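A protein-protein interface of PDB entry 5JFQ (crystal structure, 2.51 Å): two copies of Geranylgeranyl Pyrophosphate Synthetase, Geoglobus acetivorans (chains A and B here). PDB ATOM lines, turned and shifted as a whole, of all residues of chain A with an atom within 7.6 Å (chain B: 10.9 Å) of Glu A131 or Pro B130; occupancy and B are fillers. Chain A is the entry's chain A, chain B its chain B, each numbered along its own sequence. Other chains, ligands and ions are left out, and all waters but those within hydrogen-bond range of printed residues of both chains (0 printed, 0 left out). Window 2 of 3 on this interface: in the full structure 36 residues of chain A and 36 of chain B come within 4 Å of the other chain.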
ATOM      1  N   ALA A 128      -4.406 -16.166  -1.073  1.00  0.00           N
ATOM      2  CA  ALA A 128      -3.743 -16.839  -2.173  1.00  0.00           C
ATOM      3  C   ALA A 128      -2.268 -16.979  -1.802  1.00  0.00           C
ATOM      4  O   ALA A 128      -1.781 -16.246  -0.933  1.00  0.00           O
ATOM      5  CB  ALA A 128      -3.918 -16.063  -3.488  1.00  0.00           C
ATOM      6  N   PRO A 129      -1.563 -17.935  -2.402  1.00  0.00           N
ATOM      7  CA  PRO A 129      -0.148 -18.152  -2.060  1.00  0.00           C
ATOM      8  C   PRO A 129       0.694 -16.916  -2.327  1.00  0.00           C
ATOM      9  O   PRO A 129       0.588 -16.307  -3.403  1.00  0.00           O
ATOM     10  CB  PRO A 129       0.262 -19.303  -2.990  1.00  0.00           C
ATOM     11  CG  PRO A 129      -0.996 -19.995  -3.296  1.00  0.00           C
ATOM     12  CD  PRO A 129      -2.062 -18.954  -3.345  1.00  0.00           C
ATOM     13  N   PRO A 130       1.608 -16.575  -1.407  1.00  0.00           N
ATOM     14  CA  PRO A 130       2.422 -15.356  -1.566  1.00  0.00           C
ATOM     15  C   PRO A 130       3.144 -15.248  -2.894  1.00  0.00           C
ATOM     16  O   PRO A 130       3.272 -14.143  -3.443  1.00  0.00           O
ATOM     17  CB  PRO A 130       3.429 -15.461  -0.416  1.00  0.00           C
ATOM     18  CG  PRO A 130       2.857 -16.478   0.525  1.00  0.00           C
ATOM     19  CD  PRO A 130       2.112 -17.425  -0.317  1.00  0.00           C
ATOM     20  N   GLU A 131       3.647 -16.364  -3.419  1.00  0.00           N
ATOM     21  CA  GLU A 131       4.368 -16.308  -4.684  1.00  0.00           C
ATOM     22  C   GLU A 131       3.461 -15.809  -5.793  1.00  0.00           C
ATOM     23  O   GLU A 131       3.927 -15.206  -6.765  1.00  0.00           O
ATOM     24  CB  GLU A 131       4.931 -17.687  -5.044  1.00  0.00           C
ATOM     25  CG  GLU A 131       5.427 -18.484  -3.863  1.00  0.00           C
ATOM     26  CD  GLU A 131       4.334 -19.337  -3.223  1.00  0.00           C
ATOM     27  OE1 GLU A 131       3.495 -19.902  -3.975  1.00  0.00           O
ATOM     28  OE2 GLU A 131       4.317 -19.439  -1.974  1.00  0.00           O
ATOM     29  N   ASN A 132       2.167 -16.065  -5.666  1.00  0.00           N
ATOM     30  CA  ASN A 132       1.229 -15.611  -6.671  1.00  0.00           C
ATOM     31  C   ASN A 132       0.831 -14.169  -6.422  1.00  0.00           C
ATOM     32  O   ASN A 132       0.657 -13.394  -7.369  1.00  0.00           O
ATOM     33  CB  ASN A 132       0.009 -16.516  -6.675  1.00  0.00           C
ATOM     34  CG  ASN A 132       0.352 -17.919  -7.080  1.00  0.00           C
ATOM     35  OD1 ASN A 132       1.309 -18.134  -7.807  1.00  0.00           O
ATOM     36  ND2 ASN A 132      -0.405 -18.877  -6.596  1.00  0.00           N
ATOM     37  N   ILE A 133       0.680 -13.806  -5.152  1.00  0.00           N
ATOM     38  CA  ILE A 133       0.453 -12.414  -4.803  1.00  0.00           C
ATOM     39  C   ILE A 133       1.585 -11.561  -5.349  1.00  0.00           C
ATOM     40  O   ILE A 133       1.348 -10.535  -6.003  1.00  0.00           O
ATOM     41  CB  ILE A 133       0.309 -12.274  -3.282  1.00  0.00           C
ATOM     42  CG1 ILE A 133      -0.879 -13.122  -2.816  1.00  0.00           C
ATOM     43  CG2 ILE A 133       0.152 -10.841  -2.918  1.00  0.00           C
ATOM     44  CD1 ILE A 133      -1.184 -13.037  -1.354  1.00  0.00           C
ATOM     45  N   VAL A 134       2.830 -12.012  -5.147  1.00  0.00           N
ATOM     46  CA  VAL A 134       3.978 -11.242  -5.625  1.00  0.00           C
ATOM     47  C   VAL A 134       3.911 -11.082  -7.136  1.00  0.00           C
ATOM     48  O   VAL A 134       4.202 -10.002  -7.675  1.00  0.00           O
ATOM     49  CB  VAL A 134       5.306 -11.897  -5.189  1.00  0.00           C
ATOM     50  CG1 VAL A 134       6.505 -11.195  -5.855  1.00  0.00           C
ATOM     51  CG2 VAL A 134       5.452 -11.857  -3.700  1.00  0.00           C
ATOM     52  N   ARG A 135       3.507 -12.146  -7.839  1.00  0.00           N
ATOM     53  CA  ARG A 135       3.351 -12.061  -9.287  1.00  0.00           C
ATOM     54  C   ARG A 135       2.162 -11.180  -9.673  1.00  0.00           C
ATOM     55  O   ARG A 135       2.214 -10.456 -10.671  1.00  0.00           O
ATOM     56  CB  ARG A 135       3.197 -13.467  -9.878  1.00  0.00           C
ATOM     57  CG  ARG A 135       4.421 -14.356  -9.685  1.00  0.00           C
ATOM     58  CD  ARG A 135       4.137 -15.802 -10.002  1.00  0.00           C
ATOM     59  NE  ARG A 135       3.526 -15.905 -11.315  1.00  0.00           N
ATOM     60  CZ  ARG A 135       2.340 -16.465 -11.569  1.00  0.00           C
ATOM     61  NH1 ARG A 135       1.627 -17.037 -10.583  1.00  0.00           N
ATOM     62  NH2 ARG A 135       1.879 -16.465 -12.830  1.00  0.00           N
ATOM     63  N   ALA A 136       1.070 -11.247  -8.921  1.00  0.00           N
ATOM     64  CA  ALA A 136      -0.046 -10.372  -9.238  1.00  0.00           C
ATOM     65  C   ALA A 136       0.337  -8.913  -9.007  1.00  0.00           C
ATOM     66  O   ALA A 136      -0.008  -8.035  -9.806  1.00  0.00           O
ATOM     67  CB  ALA A 136      -1.267 -10.769  -8.419  1.00  0.00           C
ATOM     68  N   VAL A 137       1.104  -8.647  -7.950  1.00  0.00           N
ATOM     69  CA  VAL A 137       1.586  -7.288  -7.724  1.00  0.00           C
ATOM     70  C   VAL A 137       2.453  -6.853  -8.890  1.00  0.00           C
ATOM     71  O   VAL A 137       2.203  -5.819  -9.518  1.00  0.00           O
ATOM     72  CB  VAL A 137       2.335  -7.195  -6.387  1.00  0.00           C
ATOM     73  CG1 VAL A 137       3.132  -5.922  -6.317  1.00  0.00           C
ATOM     74  CG2 VAL A 137       1.351  -7.280  -5.242  1.00  0.00           C
ATOM     75  N   VAL A 189      -3.272 -15.836 -12.252  1.00  0.00           N
ATOM     76  CA  VAL A 189      -2.020 -15.617 -11.535  1.00  0.00           C
ATOM     77  C   VAL A 189      -2.157 -16.064 -10.088  1.00  0.00           C
ATOM     78  O   VAL A 189      -1.370 -16.883  -9.591  1.00  0.00           O
ATOM     79  CB  VAL A 189      -1.597 -14.142 -11.615  1.00  0.00           C
ATOM     80  CG1 VAL A 189      -0.259 -13.975 -10.930  1.00  0.00           C
ATOM     81  CG2 VAL A 189      -1.566 -13.661 -13.065  1.00  0.00           C
ATOM     82  N   LEU A 190      -3.172 -15.538  -9.394  1.00  0.00           N
ATOM     83  CA  LEU A 190      -3.290 -15.779  -7.960  1.00  0.00           C
ATOM     84  C   LEU A 190      -3.394 -17.262  -7.631  1.00  0.00           C
ATOM     85  O   LEU A 190      -2.905 -17.696  -6.583  1.00  0.00           O
ATOM     86  CB  LEU A 190      -4.501 -15.040  -7.398  1.00  0.00           C
ATOM     87  CG  LEU A 190      -4.342 -13.519  -7.300  1.00  0.00           C
ATOM     88  CD1 LEU A 190      -5.676 -12.900  -6.981  1.00  0.00           C
ATOM     89  CD2 LEU A 190      -3.303 -13.106  -6.272  1.00  0.00           C
ATOM     90  N   LEU B 123      10.047  -3.509  -6.186  1.00  0.00           N
ATOM     91  CA  LEU B 123       9.952  -4.168  -4.890  1.00  0.00           C
ATOM     92  C   LEU B 123       9.677  -5.657  -5.045  1.00  0.00           C
ATOM     93  O   LEU B 123      10.322  -6.482  -4.394  1.00  0.00           O
ATOM     94  CB  LEU B 123       8.861  -3.518  -4.038  1.00  0.00           C
ATOM     95  CG  LEU B 123       8.590  -4.194  -2.689  1.00  0.00           C
ATOM     96  CD1 LEU B 123       9.840  -4.238  -1.858  1.00  0.00           C
ATOM     97  CD2 LEU B 123       7.515  -3.450  -1.940  1.00  0.00           C
ATOM     98  N   SER B 124       8.745  -6.016  -5.932  1.00  0.00           N
ATOM     99  CA  SER B 124       8.299  -7.387  -6.110  1.00  0.00           C
ATOM    100  C   SER B 124       9.375  -8.281  -6.699  1.00  0.00           C
ATOM    101  O   SER B 124       9.215  -9.507  -6.675  1.00  0.00           O
ATOM    102  CB  SER B 124       7.054  -7.427  -7.002  1.00  0.00           C
ATOM    103  OG  SER B 124       7.406  -7.362  -8.381  1.00  0.00           O
ATOM    104  N   MET B 125      10.444  -7.704  -7.241  1.00  0.00           N
ATOM    105  CA  MET B 125      11.558  -8.490  -7.752  1.00  0.00           C
ATOM    106  C   MET B 125      12.474  -8.998  -6.652  1.00  0.00           C
ATOM    107  O   MET B 125      13.463  -9.669  -6.963  1.00  0.00           O
ATOM    108  CB  MET B 125      12.401  -7.669  -8.721  1.00  0.00           C
ATOM    109  CG  MET B 125      11.660  -7.074  -9.873  1.00  0.00           C
ATOM    110  SD  MET B 125      12.783  -6.003 -10.798  1.00  0.00           S
ATOM    111  CE  MET B 125      11.636  -5.125 -11.844  1.00  0.00           C
ATOM    112  N   SER B 126      12.189  -8.685  -5.388  1.00  0.00           N
ATOM    113  CA  SER B 126      13.156  -8.933  -4.330  1.00  0.00           C
ATOM    114  C   SER B 126      13.467 -10.420  -4.186  1.00  0.00           C
ATOM    115  O   SER B 126      12.590 -11.277  -4.325  1.00  0.00           O
ATOM    116  CB  SER B 126      12.648  -8.373  -3.005  1.00  0.00           C
ATOM    117  OG  SER B 126      12.787  -6.963  -2.977  1.00  0.00           O
ATOM    118  N   ASP B 127      14.739 -10.719  -3.913  1.00  0.00           N
ATOM    119  CA  ASP B 127      15.179 -12.063  -3.558  1.00  0.00           C
ATOM    120  C   ASP B 127      14.966 -12.253  -2.063  1.00  0.00           C
ATOM    121  O   ASP B 127      15.872 -12.087  -1.240  1.00  0.00           O
ATOM    122  CB  ASP B 127      16.636 -12.269  -3.938  1.00  0.00           C
ATOM    123  CG  ASP B 127      17.202 -13.564  -3.391  1.00  0.00           C
ATOM    124  OD1 ASP B 127      16.435 -14.534  -3.146  1.00  0.00           O
ATOM    125  OD2 ASP B 127      18.431 -13.594  -3.196  1.00  0.00           O
ATOM    126  N   ALA B 128      13.733 -12.593  -1.707  1.00  0.00           N
ATOM    127  CA  ALA B 128      13.380 -12.811  -0.316  1.00  0.00           C
ATOM    128  C   ALA B 128      12.152 -13.706  -0.273  1.00  0.00           C
ATOM    129  O   ALA B 128      11.473 -13.877  -1.297  1.00  0.00           O
ATOM    130  CB  ALA B 128      13.130 -11.475   0.407  1.00  0.00           C
ATOM    131  N   PRO B 129      11.862 -14.317   0.878  1.00  0.00           N
ATOM    132  CA  PRO B 129      10.633 -15.120   1.029  1.00  0.00           C
ATOM    133  C   PRO B 129       9.423 -14.370   0.507  1.00  0.00           C
ATOM    134  O   PRO B 129       9.212 -13.211   0.880  1.00  0.00           O
ATOM    135  CB  PRO B 129      10.531 -15.318   2.547  1.00  0.00           C
ATOM    136  CG  PRO B 129      11.916 -15.158   3.055  1.00  0.00           C
ATOM    137  CD  PRO B 129      12.665 -14.274   2.115  1.00  0.00           C
ATOM    138  N   PRO B 130       8.587 -14.997  -0.326  1.00  0.00           N
ATOM    139  CA  PRO B 130       7.492 -14.232  -0.971  1.00  0.00           C
ATOM    140  C   PRO B 130       6.502 -13.664   0.029  1.00  0.00           C
ATOM    141  O   PRO B 130       6.081 -12.507  -0.089  1.00  0.00           O
ATOM    142  CB  PRO B 130       6.841 -15.270  -1.896  1.00  0.00           C
ATOM    143  CG  PRO B 130       7.848 -16.422  -1.965  1.00  0.00           C
ATOM    144  CD  PRO B 130       8.547 -16.425  -0.663  1.00  0.00           C
ATOM    145  N   GLU B 131       6.096 -14.483   0.989  1.00  0.00           N
ATOM    146  CA  GLU B 131       5.457 -14.121   2.250  1.00  0.00           C
ATOM    147  C   GLU B 131       5.923 -12.768   2.784  1.00  0.00           C
ATOM    148  O   GLU B 131       5.108 -11.957   3.248  1.00  0.00           O
ATOM    149  CB  GLU B 131       5.780 -15.236   3.237  1.00  0.00           C
ATOM    150  CG  GLU B 131       7.191 -15.807   2.845  1.00  0.00           C
ATOM    151  CD  GLU B 131       7.645 -17.008   3.615  1.00  0.00           C
ATOM    152  OE1 GLU B 131       7.603 -16.998   4.864  1.00  0.00           O
ATOM    153  OE2 GLU B 131       8.056 -17.987   2.951  1.00  0.00           O
ATOM    154  N   ASN B 132       7.236 -12.520   2.733  1.00  0.00           N
ATOM    155  CA  ASN B 132       7.790 -11.258   3.212  1.00  0.00           C
ATOM    156  C   ASN B 132       7.766 -10.169   2.152  1.00  0.00           C
ATOM    157  O   ASN B 132       7.746  -8.984   2.500  1.00  0.00           O
ATOM    158  CB  ASN B 132       9.234 -11.434   3.695  1.00  0.00           C
ATOM    159  CG  ASN B 132       9.341 -12.293   4.939  1.00  0.00           C
ATOM    160  OD1 ASN B 132       8.365 -12.476   5.673  1.00  0.00           O
ATOM    161  ND2 ASN B 132      10.538 -12.798   5.202  1.00  0.00           N
ATOM    162  N   ILE B 133       7.804 -10.529   0.869  1.00  0.00           N
ATOM    163  CA  ILE B 133       7.601  -9.514  -0.156  1.00  0.00           C
ATOM    164  C   ILE B 133       6.179  -8.975  -0.068  1.00  0.00           C
ATOM    165  O   ILE B 133       5.947  -7.762  -0.181  1.00  0.00           O
ATOM    166  CB  ILE B 133       7.915 -10.088  -1.548  1.00  0.00           C
ATOM    167  CG1 ILE B 133       9.263 -10.818  -1.549  1.00  0.00           C
ATOM    168  CG2 ILE B 133       7.947  -8.982  -2.571  1.00  0.00           C
ATOM    169  CD1 ILE B 133       9.707 -11.234  -2.935  1.00  0.00           C
ATOM    170  N   VAL B 134       5.208  -9.866   0.171  1.00  0.00           N
ATOM    171  CA  VAL B 134       3.820  -9.442   0.339  1.00  0.00           C
ATOM    172  C   VAL B 134       3.709  -8.442   1.479  1.00  0.00           C
ATOM    173  O   VAL B 134       3.196  -7.333   1.302  1.00  0.00           O
ATOM    174  CB  VAL B 134       2.904 -10.654   0.562  1.00  0.00           C
ATOM    175  CG1 VAL B 134       1.503 -10.172   0.907  1.00  0.00           C
ATOM    176  CG2 VAL B 134       2.876 -11.501  -0.676  1.00  0.00           C
ATOM    177  N   ARG B 135       4.218  -8.807   2.657  1.00  0.00           N
ATOM    178  CA  ARG B 135       4.227  -7.868   3.772  1.00  0.00           C
ATOM    179  C   ARG B 135       4.948  -6.568   3.421  1.00  0.00           C
ATOM    180  O   ARG B 135       4.514  -5.490   3.835  1.00  0.00           O
ATOM    181  CB  ARG B 135       4.853  -8.515   4.998  1.00  0.00           C
ATOM    182  CG  ARG B 135       3.909  -9.460   5.725  1.00  0.00           C
ATOM    183  CD  ARG B 135       4.650 -10.279   6.775  1.00  0.00           C
ATOM    184  NE  ARG B 135       5.359  -9.453   7.755  1.00  0.00           N
ATOM    185  CZ  ARG B 135       6.639  -9.621   8.089  1.00  0.00           C
ATOM    186  NH1 ARG B 135       7.365 -10.592   7.529  1.00  0.00           N
ATOM    187  NH2 ARG B 135       7.189  -8.833   9.003  1.00  0.00           N
ATOM    188  N   ALA B 136       6.039  -6.642   2.656  1.00  0.00           N
ATOM    189  CA  ALA B 136       6.755  -5.430   2.271  1.00  0.00           C
ATOM    190  C   ALA B 136       5.920  -4.578   1.335  1.00  0.00           C
ATOM    191  O   ALA B 136       5.918  -3.346   1.441  1.00  0.00           O
ATOM    192  CB  ALA B 136       8.091  -5.770   1.612  1.00  0.00           C
ATOM    193  N   VAL B 137       5.209  -5.210   0.404  1.00  0.00           N
ATOM    194  CA  VAL B 137       4.335  -4.441  -0.472  1.00  0.00           C
ATOM    195  C   VAL B 137       3.222  -3.780   0.339  1.00  0.00           C
ATOM    196  O   VAL B 137       2.911  -2.596   0.150  1.00  0.00           O
ATOM    197  CB  VAL B 137       3.790  -5.348  -1.589  1.00  0.00           C
ATOM    198  CG1 VAL B 137       2.600  -4.702  -2.281  1.00  0.00           C
ATOM    199  CG2 VAL B 137       4.893  -5.667  -2.580  1.00  0.00           C
ATOM    200  N   SER B 138       2.643  -4.520   1.286  1.00  0.00           N
ATOM    201  CA  SER B 138       1.560  -3.993   2.107  1.00  0.00           C
ATOM    202  C   SER B 138       2.013  -2.799   2.943  1.00  0.00           C
ATOM    203  O   SER B 138       1.296  -1.785   3.053  1.00  0.00           O
ATOM    204  CB  SER B 138       1.027  -5.095   3.017  1.00  0.00           C
ATOM    205  OG  SER B 138       0.101  -4.566   3.946  1.00  0.00           O
ATOM    206  N   LYS B 139       3.204  -2.906   3.544  1.00  0.00           N
ATOM    207  CA  LYS B 139       3.713  -1.844   4.399  1.00  0.00           C
ATOM    208  C   LYS B 139       4.101  -0.607   3.590  1.00  0.00           C
ATOM    209  O   LYS B 139       3.782   0.521   3.982  1.00  0.00           O
ATOM    210  CB  LYS B 139       4.877  -2.390   5.216  1.00  0.00           C
ATOM    211  CG  LYS B 139       4.412  -3.419   6.278  1.00  0.00           C
ATOM    212  CD  LYS B 139       5.568  -4.270   6.808  1.00  0.00           C
ATOM    213  CE  LYS B 139       5.097  -5.374   7.760  1.00  0.00           C
ATOM    214  NZ  LYS B 139       4.740  -4.930   9.142  1.00  0.00           N
ATOM    215  N   ILE B 186      12.351  -1.952   6.118  1.00  0.00           N
ATOM    216  CA  ILE B 186      11.973  -2.960   5.127  1.00  0.00           C
ATOM    217  C   ILE B 186      12.926  -4.155   5.093  1.00  0.00           C
ATOM    218  O   ILE B 186      12.450  -5.272   4.842  1.00  0.00           O
ATOM    219  CB  ILE B 186      11.773  -2.341   3.728  1.00  0.00           C
ATOM    220  CG1 ILE B 186      10.926  -3.286   2.861  1.00  0.00           C
ATOM    221  CG2 ILE B 186      13.081  -1.963   3.039  1.00  0.00           C
ATOM    222  CD1 ILE B 186      10.662  -2.776   1.445  1.00  0.00           C
ATOM    223  N   VAL B 189      11.631  -6.547   7.398  1.00  0.00           N
ATOM    224  CA  VAL B 189      10.452  -7.212   6.871  1.00  0.00           C
ATOM    225  C   VAL B 189      10.853  -8.256   5.849  1.00  0.00           C
ATOM    226  O   VAL B 189      10.356  -9.387   5.871  1.00  0.00           O
ATOM    227  CB  VAL B 189       9.478  -6.194   6.266  1.00  0.00           C
ATOM    228  CG1 VAL B 189       8.213  -6.905   5.806  1.00  0.00           C
ATOM    229  CG2 VAL B 189       9.164  -5.121   7.276  1.00  0.00           C
ATOM    230  N   LEU B 190      11.768  -7.891   4.944  1.00  0.00           N
ATOM    231  CA  LEU B 190      12.119  -8.771   3.836  1.00  0.00           C
ATOM    232  C   LEU B 190      12.775 -10.062   4.324  1.00  0.00           C
ATOM    233  O   LEU B 190      12.547 -11.133   3.755  1.00  0.00           O
ATOM    234  CB  LEU B 190      13.030  -8.033   2.853  1.00  0.00           C
ATOM    235  CG  LEU B 190      12.282  -7.114   1.879  1.00  0.00           C
ATOM    236  CD1 LEU B 190      13.206  -6.280   0.993  1.00  0.00           C
ATOM    237  CD2 LEU B 190      11.339  -7.946   1.034  1.00  0.00           C
ATOM    238  N   PHE B 191      13.574  -9.983   5.386  1.00  0.00           N
ATOM    239  CA  PHE B 191      14.353 -11.108   5.887  1.00  0.00           C
ATOM    240  C   PHE B 191      13.862 -11.578   7.247  1.00  0.00           C
ATOM    241  O   PHE B 191      14.652 -12.004   8.087  1.00  0.00           O
ATOM    242  CB  PHE B 191      15.826 -10.728   5.938  1.00  0.00           C
ATOM    243  CG  PHE B 191      16.281 -10.080   4.693  1.00  0.00           C
ATOM    244  CD1 PHE B 191      15.816 -10.531   3.470  1.00  0.00           C
ATOM    245  CD2 PHE B 191      17.121  -8.995   4.724  1.00  0.00           C
ATOM    246  CE1 PHE B 191      16.203  -9.932   2.290  1.00  0.00           C
ATOM    247  CE2 PHE B 191      17.518  -8.385   3.548  1.00  0.00           C
ATOM    248  CZ  PHE B 191      17.051  -8.858   2.325  1.00  0.00           C
ATOM    249  N   GLY B 192      12.562 -11.466   7.485  1.00  0.00           N
ATOM    250  CA  GLY B 192      11.947 -12.193   8.573  1.00  0.00           C
ATOM    251  C   GLY B 192      12.504 -11.916   9.949  1.00  0.00           C
ATOM    252  O   GLY B 192      12.352 -12.753  10.842  1.00  0.00           O
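Pro B130 touches its own counterpart, Pro A130. Pro A130 touches Glu B131, and with the chains exchanged Glu A131 touches Pro B130. Pro A130 touches Val B134, and with the chains exchanged Val A134 touches Pro B130. Val A134 touches its own counterpart, Val B134. Of the 9 pairs that touch across the chains among the printed residues, 8 have their exchanged pair printed and touching as well.
Among the printed residues, pairs that only touch across the chains: Pro A130 with Glu B131 (3.2 Å), Val A134 with Ser B124 (3.3 Å), Pro A130 with Pro B130 (3.6 Å), Ile A133 with Val B134 (3.6 Å), Glu A131 with Pro B130 (3.7 Å), Val A134 with Ile B133 (3.7 Å), Val A134 with Pro B130 (3.7 Å), Pro A130 with Val B134 (3.8 Å) and Val A134 with Val B134 (3.99 Å).
Of the 22 printed residues of chain B, 5 touch a printed residue of chain A. Printed residues of chain B that touch a printed residue of chain A: Ser B124, Pro B130, Glu B131, Ile B133 and Val B134. Hydrophobic or aromatic side chains of chain B that line the printed part of chain A: Pro B130, Ile B133 and Val B134. Hydrophobic or aromatic side chains of chain A within 4 Å of the printed part of chain B: Pro A130, Ile A133 and Val A134. Among the printed residues, 9 pairs touch across the chains. Among the printed residues, no Asp or Glu carboxylate lies within 4 Å of a Lys or Arg side-chain nitrogen of the other chain.
Pro A130 touches three residues of chain B. Of chain B, only Pro B130 comes within 4 Å of Glu A131. No residue of chain B comes within 4 Å of Asn A132. Ile A133 touches one residue of chain B. Of the printed residues of chain B, Val A134 touches Ser B124, Pro B130, Ile B133 and Val B134. No residue of chain B comes within 4 Å of Arg A135. Of the printed residues of chain A, Ser B124 touches Val A134. Of chain A, only Pro A130, Glu A131 and Val A134 come within 4 Å of Pro B130. Of the printed residues of chain A, Glu B131 touches Pro A130 (3.2 Å). Of the printed residues of chain A, Ile B133 touches Val A134. Printed residues of chain A within 4 Å of Val B134: Pro A130 (3.8 Å), Ile A133 (3.6 Å) and Val A134 (3.99 Å). Phe B191 touches none of the printed residues of chain A. Gly B192 touches none of the printed residues of chain A. The nearest residue of chain B that does not touch Glu A131 is Glu B131 (5.4 Å).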
